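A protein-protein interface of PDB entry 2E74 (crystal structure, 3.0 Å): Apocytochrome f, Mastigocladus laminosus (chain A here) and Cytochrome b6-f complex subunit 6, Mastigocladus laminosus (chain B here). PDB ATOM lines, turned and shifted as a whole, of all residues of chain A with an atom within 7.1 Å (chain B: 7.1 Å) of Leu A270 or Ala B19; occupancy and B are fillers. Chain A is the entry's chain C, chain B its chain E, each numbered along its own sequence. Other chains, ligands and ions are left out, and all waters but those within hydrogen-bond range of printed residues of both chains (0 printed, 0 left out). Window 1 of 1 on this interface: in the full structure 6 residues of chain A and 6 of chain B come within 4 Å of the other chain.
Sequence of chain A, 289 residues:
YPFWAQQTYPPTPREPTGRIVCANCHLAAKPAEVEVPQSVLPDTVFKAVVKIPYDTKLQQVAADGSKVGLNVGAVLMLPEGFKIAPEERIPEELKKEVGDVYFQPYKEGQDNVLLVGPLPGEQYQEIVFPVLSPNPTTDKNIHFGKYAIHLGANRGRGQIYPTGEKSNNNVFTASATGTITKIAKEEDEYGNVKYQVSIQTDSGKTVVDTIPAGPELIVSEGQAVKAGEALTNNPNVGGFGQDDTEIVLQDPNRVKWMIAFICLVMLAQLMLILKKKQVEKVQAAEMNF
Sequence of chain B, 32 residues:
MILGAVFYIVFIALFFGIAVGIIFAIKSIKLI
CE of Met A266 touches CE1 of Phe B15, 3.7 Å away.
CD1 of Leu A270 touches CA of Ala B19, at 3.95 Å.
Ile B22 touches Leu A274 (CG2 to CD1, 3.2 Å).
Leu A270 touches just one residue of chain B: Ala B19.
Ala B19 touches just one residue of chain A: Leu A270 (3.95 Å).
Of the printed residues of chain B, Met A266 touches Phe B15 (3.7 Å).
Printed residues of chain A within 4 Å of Ile B22: Leu A274 (3.2 Å).
Of the printed residues of chain A, Phe B15 touches Met A266 (3.7 Å).
Leu A264 touches none of the printed residues of chain B.
Leu A267 touches none of the printed residues of chain B.
The nearest printed residue of chain B that does not touch Leu A274 is Ile B23 (4.4 Å).
Hydrophobic or aromatic side chains of chain B that line the printed part of chain A: Phe B15 and Ile B22.
Printed residues of chain A that touch a printed residue of chain B: Met A266, Leu A270 and Leu A274.
Among the printed residues, 3 pairs touch across the chains.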
ATOM      1  N   LEU A 264     -33.999 -29.394  13.901  1.00  0.00           N
ATOM      2  CA  LEU A 264     -33.972 -28.205  14.736  1.00  0.00           C
ATOM      3  C   LEU A 264     -32.522 -27.970  15.162  1.00  0.00           C
ATOM      4  O   LEU A 264     -31.997 -26.859  15.061  1.00  0.00           O
ATOM      5  CB  LEU A 264     -34.867 -28.374  15.961  1.00  0.00           C
ATOM      6  CG  LEU A 264     -35.727 -27.154  16.319  1.00  0.00           C
ATOM      7  CD1 LEU A 264     -36.195 -27.182  17.770  1.00  0.00           C
ATOM      8  CD2 LEU A 264     -34.943 -25.899  16.064  1.00  0.00           C
ATOM      9  N   VAL A 265     -31.860 -29.033  15.599  1.00  0.00           N
ATOM     10  CA  VAL A 265     -30.497 -28.915  16.099  1.00  0.00           C
ATOM     11  C   VAL A 265     -29.560 -28.352  15.037  1.00  0.00           C
ATOM     12  O   VAL A 265     -28.722 -27.515  15.342  1.00  0.00           O
ATOM     13  CB  VAL A 265     -29.933 -30.263  16.616  1.00  0.00           C
ATOM     14  CG1 VAL A 265     -28.494 -30.114  16.934  1.00  0.00           C
ATOM     15  CG2 VAL A 265     -30.666 -30.740  17.853  1.00  0.00           C
ATOM     16  N   MET A 266     -29.690 -28.803  13.793  1.00  0.00           N
ATOM     17  CA  MET A 266     -28.740 -28.360  12.761  1.00  0.00           C
ATOM     18  C   MET A 266     -28.986 -26.901  12.442  1.00  0.00           C
ATOM     19  O   MET A 266     -28.058 -26.089  12.360  1.00  0.00           O
ATOM     20  CB  MET A 266     -28.840 -29.212  11.508  1.00  0.00           C
ATOM     21  CG  MET A 266     -28.538 -30.661  11.765  1.00  0.00           C
ATOM     22  SD  MET A 266     -28.617 -31.595  10.240  1.00  0.00           S
ATOM     23  CE  MET A 266     -30.385 -31.806  10.139  1.00  0.00           C
ATOM     24  N   LEU A 267     -30.263 -26.592  12.283  1.00  0.00           N
ATOM     25  CA  LEU A 267     -30.754 -25.243  12.139  1.00  0.00           C
ATOM     26  C   LEU A 267     -30.162 -24.382  13.248  1.00  0.00           C
ATOM     27  O   LEU A 267     -29.591 -23.325  12.995  1.00  0.00           O
ATOM     28  CB  LEU A 267     -32.282 -25.280  12.257  1.00  0.00           C
ATOM     29  CG  LEU A 267     -33.099 -24.513  11.229  1.00  0.00           C
ATOM     30  CD1 LEU A 267     -33.824 -23.314  11.862  1.00  0.00           C
ATOM     31  CD2 LEU A 267     -32.157 -24.103  10.101  1.00  0.00           C
ATOM     32  N   ALA A 268     -30.285 -24.831  14.490  1.00  0.00           N
ATOM     33  CA  ALA A 268     -29.779 -24.015  15.583  1.00  0.00           C
ATOM     34  C   ALA A 268     -28.268 -23.874  15.495  1.00  0.00           C
ATOM     35  O   ALA A 268     -27.721 -22.801  15.753  1.00  0.00           O
ATOM     36  CB  ALA A 268     -30.184 -24.571  16.908  1.00  0.00           C
ATOM     37  N   GLN A 269     -27.581 -24.941  15.123  1.00  0.00           N
ATOM     38  CA  GLN A 269     -26.137 -24.835  15.007  1.00  0.00           C
ATOM     39  C   GLN A 269     -25.760 -23.762  13.989  1.00  0.00           C
ATOM     40  O   GLN A 269     -24.844 -22.964  14.214  1.00  0.00           O
ATOM     41  CB  GLN A 269     -25.519 -26.174  14.632  1.00  0.00           C
ATOM     42  CG  GLN A 269     -25.490 -27.144  15.778  1.00  0.00           C
ATOM     43  CD  GLN A 269     -25.289 -28.542  15.298  1.00  0.00           C
ATOM     44  OE1 GLN A 269     -25.836 -28.912  14.269  1.00  0.00           O
ATOM     45  NE2 GLN A 269     -24.492 -29.330  16.023  1.00  0.00           N
ATOM     46  N   LEU A 270     -26.478 -23.749  12.870  1.00  0.00           N
ATOM     47  CA  LEU A 270     -26.174 -22.841  11.777  1.00  0.00           C
ATOM     48  C   LEU A 270     -26.265 -21.432  12.315  1.00  0.00           C
ATOM     49  O   LEU A 270     -25.367 -20.610  12.096  1.00  0.00           O
ATOM     50  CB  LEU A 270     -27.215 -22.997  10.682  1.00  0.00           C
ATOM     51  CG  LEU A 270     -26.808 -22.883   9.227  1.00  0.00           C
ATOM     52  CD1 LEU A 270     -28.067 -22.926   8.425  1.00  0.00           C
ATOM     53  CD2 LEU A 270     -25.991 -21.628   8.913  1.00  0.00           C
ATOM     54  N   MET A 271     -27.358 -21.164  13.028  1.00  0.00           N
ATOM     55  CA  MET A 271     -27.619 -19.835  13.537  1.00  0.00           C
ATOM     56  C   MET A 271     -26.502 -19.345  14.449  1.00  0.00           C
ATOM     57  O   MET A 271     -26.035 -18.213  14.319  1.00  0.00           O
ATOM     58  CB  MET A 271     -28.951 -19.805  14.255  1.00  0.00           C
ATOM     59  CG  MET A 271     -30.072 -19.177  13.458  1.00  0.00           C
ATOM     60  SD  MET A 271     -29.912 -19.363  11.682  1.00  0.00           S
ATOM     61  CE  MET A 271     -31.365 -18.471  11.132  1.00  0.00           C
ATOM     62  N   LEU A 272     -26.045 -20.192  15.359  1.00  0.00           N
ATOM     63  CA  LEU A 272     -24.891 -19.822  16.163  1.00  0.00           C
ATOM     64  C   LEU A 272     -23.673 -19.431  15.299  1.00  0.00           C
ATOM     65  O   LEU A 272     -23.090 -18.362  15.500  1.00  0.00           O
ATOM     66  CB  LEU A 272     -24.546 -20.939  17.129  1.00  0.00           C
ATOM     67  CG  LEU A 272     -25.588 -21.078  18.234  1.00  0.00           C
ATOM     68  CD1 LEU A 272     -25.304 -22.293  19.070  1.00  0.00           C
ATOM     69  CD2 LEU A 272     -25.571 -19.828  19.093  1.00  0.00           C
ATOM     70  N   ILE A 273     -23.294 -20.262  14.324  1.00  0.00           N
ATOM     71  CA  ILE A 273     -22.135 -19.925  13.496  1.00  0.00           C
ATOM     72  C   ILE A 273     -22.369 -18.632  12.727  1.00  0.00           C
ATOM     73  O   ILE A 273     -21.517 -17.730  12.741  1.00  0.00           O
ATOM     74  CB  ILE A 273     -21.770 -21.013  12.473  1.00  0.00           C
ATOM     75  CG1 ILE A 273     -21.640 -22.390  13.136  1.00  0.00           C
ATOM     76  CG2 ILE A 273     -20.501 -20.607  11.671  1.00  0.00           C
ATOM     77  CD1 ILE A 273     -20.752 -22.403  14.338  1.00  0.00           C
ATOM     78  N   LEU A 274     -23.506 -18.536  12.036  1.00  0.00           N
ATOM     79  CA  LEU A 274     -23.799 -17.299  11.313  1.00  0.00           C
ATOM     80  C   LEU A 274     -23.586 -16.140  12.265  1.00  0.00           C
ATOM     81  O   LEU A 274     -22.958 -15.142  11.915  1.00  0.00           O
ATOM     82  CB  LEU A 274     -25.223 -17.286  10.771  1.00  0.00           C
ATOM     83  CG  LEU A 274     -25.396 -18.163   9.535  1.00  0.00           C
ATOM     84  CD1 LEU A 274     -26.854 -18.220   9.130  1.00  0.00           C
ATOM     85  CD2 LEU A 274     -24.526 -17.682   8.362  1.00  0.00           C
ATOM     86  N   LYS A 275     -24.090 -16.295  13.488  1.00  0.00           N
ATOM     87  CA  LYS A 275     -23.940 -15.263  14.489  1.00  0.00           C
ATOM     88  C   LYS A 275     -22.461 -14.981  14.696  1.00  0.00           C
ATOM     89  O   LYS A 275     -22.023 -13.825  14.597  1.00  0.00           O
ATOM     90  CB  LYS A 275     -24.610 -15.669  15.803  1.00  0.00           C
ATOM     91  CG  LYS A 275     -24.521 -14.622  16.908  1.00  0.00           C
ATOM     92  CD  LYS A 275     -24.986 -13.235  16.445  1.00  0.00           C
ATOM     93  CE  LYS A 275     -24.583 -12.190  17.486  1.00  0.00           C
ATOM     94  NZ  LYS A 275     -25.000 -10.784  17.188  1.00  0.00           N
ATOM     95  N   LYS A 276     -21.685 -16.031  14.970  1.00  0.00           N
ATOM     96  CA  LYS A 276     -20.260 -15.831  15.235  1.00  0.00           C
ATOM     97  C   LYS A 276     -19.645 -14.959  14.143  1.00  0.00           C
ATOM     98  O   LYS A 276     -18.862 -14.049  14.409  1.00  0.00           O
ATOM     99  CB  LYS A 276     -19.504 -17.154  15.341  1.00  0.00           C
ATOM    100  CG  LYS A 276     -18.036 -16.943  15.650  1.00  0.00           C
ATOM    101  CD  LYS A 276     -17.271 -18.241  15.986  1.00  0.00           C
ATOM    102  CE  LYS A 276     -15.734 -17.956  15.946  1.00  0.00           C
ATOM    103  NZ  LYS A 276     -14.843 -19.119  16.258  1.00  0.00           N
ATOM    104  N   ALA B  13     -27.071 -31.655   1.263  1.00  0.00           N
ATOM    105  CA  ALA B  13     -27.131 -30.649   0.204  1.00  0.00           C
ATOM    106  C   ALA B  13     -28.217 -29.650   0.515  1.00  0.00           C
ATOM    107  O   ALA B  13     -28.038 -28.430   0.451  1.00  0.00           O
ATOM    108  CB  ALA B  13     -27.429 -31.324  -1.106  1.00  0.00           C
ATOM    109  N   LEU B  14     -29.366 -30.188   0.862  1.00  0.00           N
ATOM    110  CA  LEU B  14     -30.478 -29.356   1.236  1.00  0.00           C
ATOM    111  C   LEU B  14     -30.078 -28.327   2.314  1.00  0.00           C
ATOM    112  O   LEU B  14     -30.398 -27.134   2.218  1.00  0.00           O
ATOM    113  CB  LEU B  14     -31.620 -30.246   1.691  1.00  0.00           C
ATOM    114  CG  LEU B  14     -32.914 -29.524   1.420  1.00  0.00           C
ATOM    115  CD1 LEU B  14     -34.028 -30.552   1.231  1.00  0.00           C
ATOM    116  CD2 LEU B  14     -33.184 -28.525   2.557  1.00  0.00           C
ATOM    117  N   PHE B  15     -29.355 -28.788   3.330  1.00  0.00           N
ATOM    118  CA  PHE B  15     -28.980 -27.904   4.439  1.00  0.00           C
ATOM    119  C   PHE B  15     -27.808 -27.003   4.077  1.00  0.00           C
ATOM    120  O   PHE B  15     -27.821 -25.800   4.378  1.00  0.00           O
ATOM    121  CB  PHE B  15     -28.700 -28.699   5.732  1.00  0.00           C
ATOM    122  CG  PHE B  15     -29.885 -28.781   6.653  1.00  0.00           C
ATOM    123  CD1 PHE B  15     -30.789 -29.828   6.547  1.00  0.00           C
ATOM    124  CD2 PHE B  15     -30.107 -27.793   7.598  1.00  0.00           C
ATOM    125  CE1 PHE B  15     -31.879 -29.893   7.368  1.00  0.00           C
ATOM    126  CE2 PHE B  15     -31.203 -27.844   8.424  1.00  0.00           C
ATOM    127  CZ  PHE B  15     -32.092 -28.897   8.315  1.00  0.00           C
ATOM    128  N   PHE B  16     -26.803 -27.602   3.440  1.00  0.00           N
ATOM    129  CA  PHE B  16     -25.716 -26.849   2.843  1.00  0.00           C
ATOM    130  C   PHE B  16     -26.332 -25.696   2.095  1.00  0.00           C
ATOM    131  O   PHE B  16     -25.919 -24.545   2.268  1.00  0.00           O
ATOM    132  CB  PHE B  16     -24.923 -27.705   1.865  1.00  0.00           C
ATOM    133  CG  PHE B  16     -23.679 -27.037   1.370  1.00  0.00           C
ATOM    134  CD1 PHE B  16     -23.742 -25.812   0.736  1.00  0.00           C
ATOM    135  CD2 PHE B  16     -22.440 -27.626   1.550  1.00  0.00           C
ATOM    136  CE1 PHE B  16     -22.596 -25.186   0.287  1.00  0.00           C
ATOM    137  CE2 PHE B  16     -21.287 -27.004   1.103  1.00  0.00           C
ATOM    138  CZ  PHE B  16     -21.365 -25.789   0.470  1.00  0.00           C
ATOM    139  N   GLY B  17     -27.336 -26.013   1.274  1.00  0.00           N
ATOM    140  CA  GLY B  17     -28.093 -25.000   0.558  1.00  0.00           C
ATOM    141  C   GLY B  17     -28.519 -23.860   1.469  1.00  0.00           C
ATOM    142  O   GLY B  17     -28.138 -22.705   1.268  1.00  0.00           O
ATOM    143  N   ILE B  18     -29.302 -24.190   2.487  1.00  0.00           N
ATOM    144  CA  ILE B  18     -29.837 -23.171   3.372  1.00  0.00           C
ATOM    145  C   ILE B  18     -28.717 -22.357   3.997  1.00  0.00           C
ATOM    146  O   ILE B  18     -28.881 -21.162   4.270  1.00  0.00           O
ATOM    147  CB  ILE B  18     -30.670 -23.798   4.497  1.00  0.00           C
ATOM    148  CG1 ILE B  18     -31.727 -24.752   3.917  1.00  0.00           C
ATOM    149  CG2 ILE B  18     -31.262 -22.702   5.419  1.00  0.00           C
ATOM    150  CD1 ILE B  18     -32.704 -25.260   4.952  1.00  0.00           C
ATOM    151  N   ALA B  19     -27.585 -23.016   4.240  1.00  0.00           N
ATOM    152  CA  ALA B  19     -26.444 -22.360   4.868  1.00  0.00           C
ATOM    153  C   ALA B  19     -26.002 -21.242   3.963  1.00  0.00           C
ATOM    154  O   ALA B  19     -26.111 -20.066   4.319  1.00  0.00           O
ATOM    155  CB  ALA B  19     -25.325 -23.330   5.064  1.00  0.00           C
ATOM    156  N   VAL B  20     -25.528 -21.627   2.776  1.00  0.00           N
ATOM    157  CA  VAL B  20     -25.084 -20.687   1.748  1.00  0.00           C
ATOM    158  C   VAL B  20     -26.136 -19.634   1.455  1.00  0.00           C
ATOM    159  O   VAL B  20     -25.870 -18.430   1.520  1.00  0.00           O
ATOM    160  CB  VAL B  20     -24.833 -21.399   0.449  1.00  0.00           C
ATOM    161  CG1 VAL B  20     -24.705 -20.366  -0.649  1.00  0.00           C
ATOM    162  CG2 VAL B  20     -23.585 -22.307   0.558  1.00  0.00           C
ATOM    163  N   GLY B  21     -27.338 -20.096   1.127  1.00  0.00           N
ATOM    164  CA  GLY B  21     -28.464 -19.198   0.966  1.00  0.00           C
ATOM    165  C   GLY B  21     -28.482 -18.149   2.062  1.00  0.00           C
ATOM    166  O   GLY B  21     -28.474 -16.942   1.797  1.00  0.00           O
ATOM    167  N   ILE B  22     -28.496 -18.601   3.309  1.00  0.00           N
ATOM    168  CA  ILE B  22     -28.627 -17.661   4.408  1.00  0.00           C
ATOM    169  C   ILE B  22     -27.441 -16.691   4.499  1.00  0.00           C
ATOM    170  O   ILE B  22     -27.647 -15.533   4.879  1.00  0.00           O
ATOM    171  CB  ILE B  22     -28.909 -18.356   5.767  1.00  0.00           C
ATOM    172  CG1 ILE B  22     -30.306 -18.949   5.778  1.00  0.00           C
ATOM    173  CG2 ILE B  22     -28.937 -17.329   6.878  1.00  0.00           C
ATOM    174  CD1 ILE B  22     -31.371 -17.898   6.095  1.00  0.00           C
ATOM    175  N   ILE B  23     -26.222 -17.129   4.148  1.00  0.00           N
ATOM    176  CA  ILE B  23     -25.074 -16.217   4.272  1.00  0.00           C
ATOM    177  C   ILE B  23     -25.391 -14.987   3.469  1.00  0.00           C
ATOM    178  O   ILE B  23     -25.491 -13.886   4.009  1.00  0.00           O
ATOM    179  CB  ILE B  23     -23.731 -16.715   3.670  1.00  0.00           C
ATOM    180  CG1 ILE B  23     -23.515 -18.214   3.815  1.00  0.00           C
ATOM    181  CG2 ILE B  23     -22.530 -15.966   4.289  1.00  0.00           C
ATOM    182  CD1 ILE B  23     -22.111 -18.611   3.320  1.00  0.00           C
ATOM    183  N   PHE B  24     -25.545 -15.190   2.162  1.00  0.00           N
ATOM    184  CA  PHE B  24     -25.719 -14.084   1.239  1.00  0.00           C
ATOM    185  C   PHE B  24     -26.963 -13.275   1.555  1.00  0.00           C
ATOM    186  O   PHE B  24     -26.861 -12.089   1.852  1.00  0.00           O
ATOM    187  CB  PHE B  24     -25.661 -14.570  -0.206  1.00  0.00           C
ATOM    188  CG  PHE B  24     -24.328 -15.155  -0.567  1.00  0.00           C
ATOM    189  CD1 PHE B  24     -24.211 -16.483  -0.957  1.00  0.00           C
ATOM    190  CD2 PHE B  24     -23.168 -14.379  -0.457  1.00  0.00           C
ATOM    191  CE1 PHE B  24     -22.969 -17.026  -1.262  1.00  0.00           C
ATOM    192  CE2 PHE B  24     -21.923 -14.907  -0.759  1.00  0.00           C
ATOM    193  CZ  PHE B  24     -21.823 -16.238  -1.161  1.00  0.00           C
ATOM    194  N   ALA B  25     -28.132 -13.899   1.538  1.00  0.00           N
ATOM    195  CA  ALA B  25     -29.323 -13.154   1.913  1.00  0.00           C
ATOM    196  C   ALA B  25     -28.983 -12.320   3.157  1.00  0.00           C
ATOM    197  O   ALA B  25     -29.213 -11.109   3.211  1.00  0.00           O
ATOM    198  CB  ALA B  25     -30.478 -14.092   2.177  1.00  0.00           C
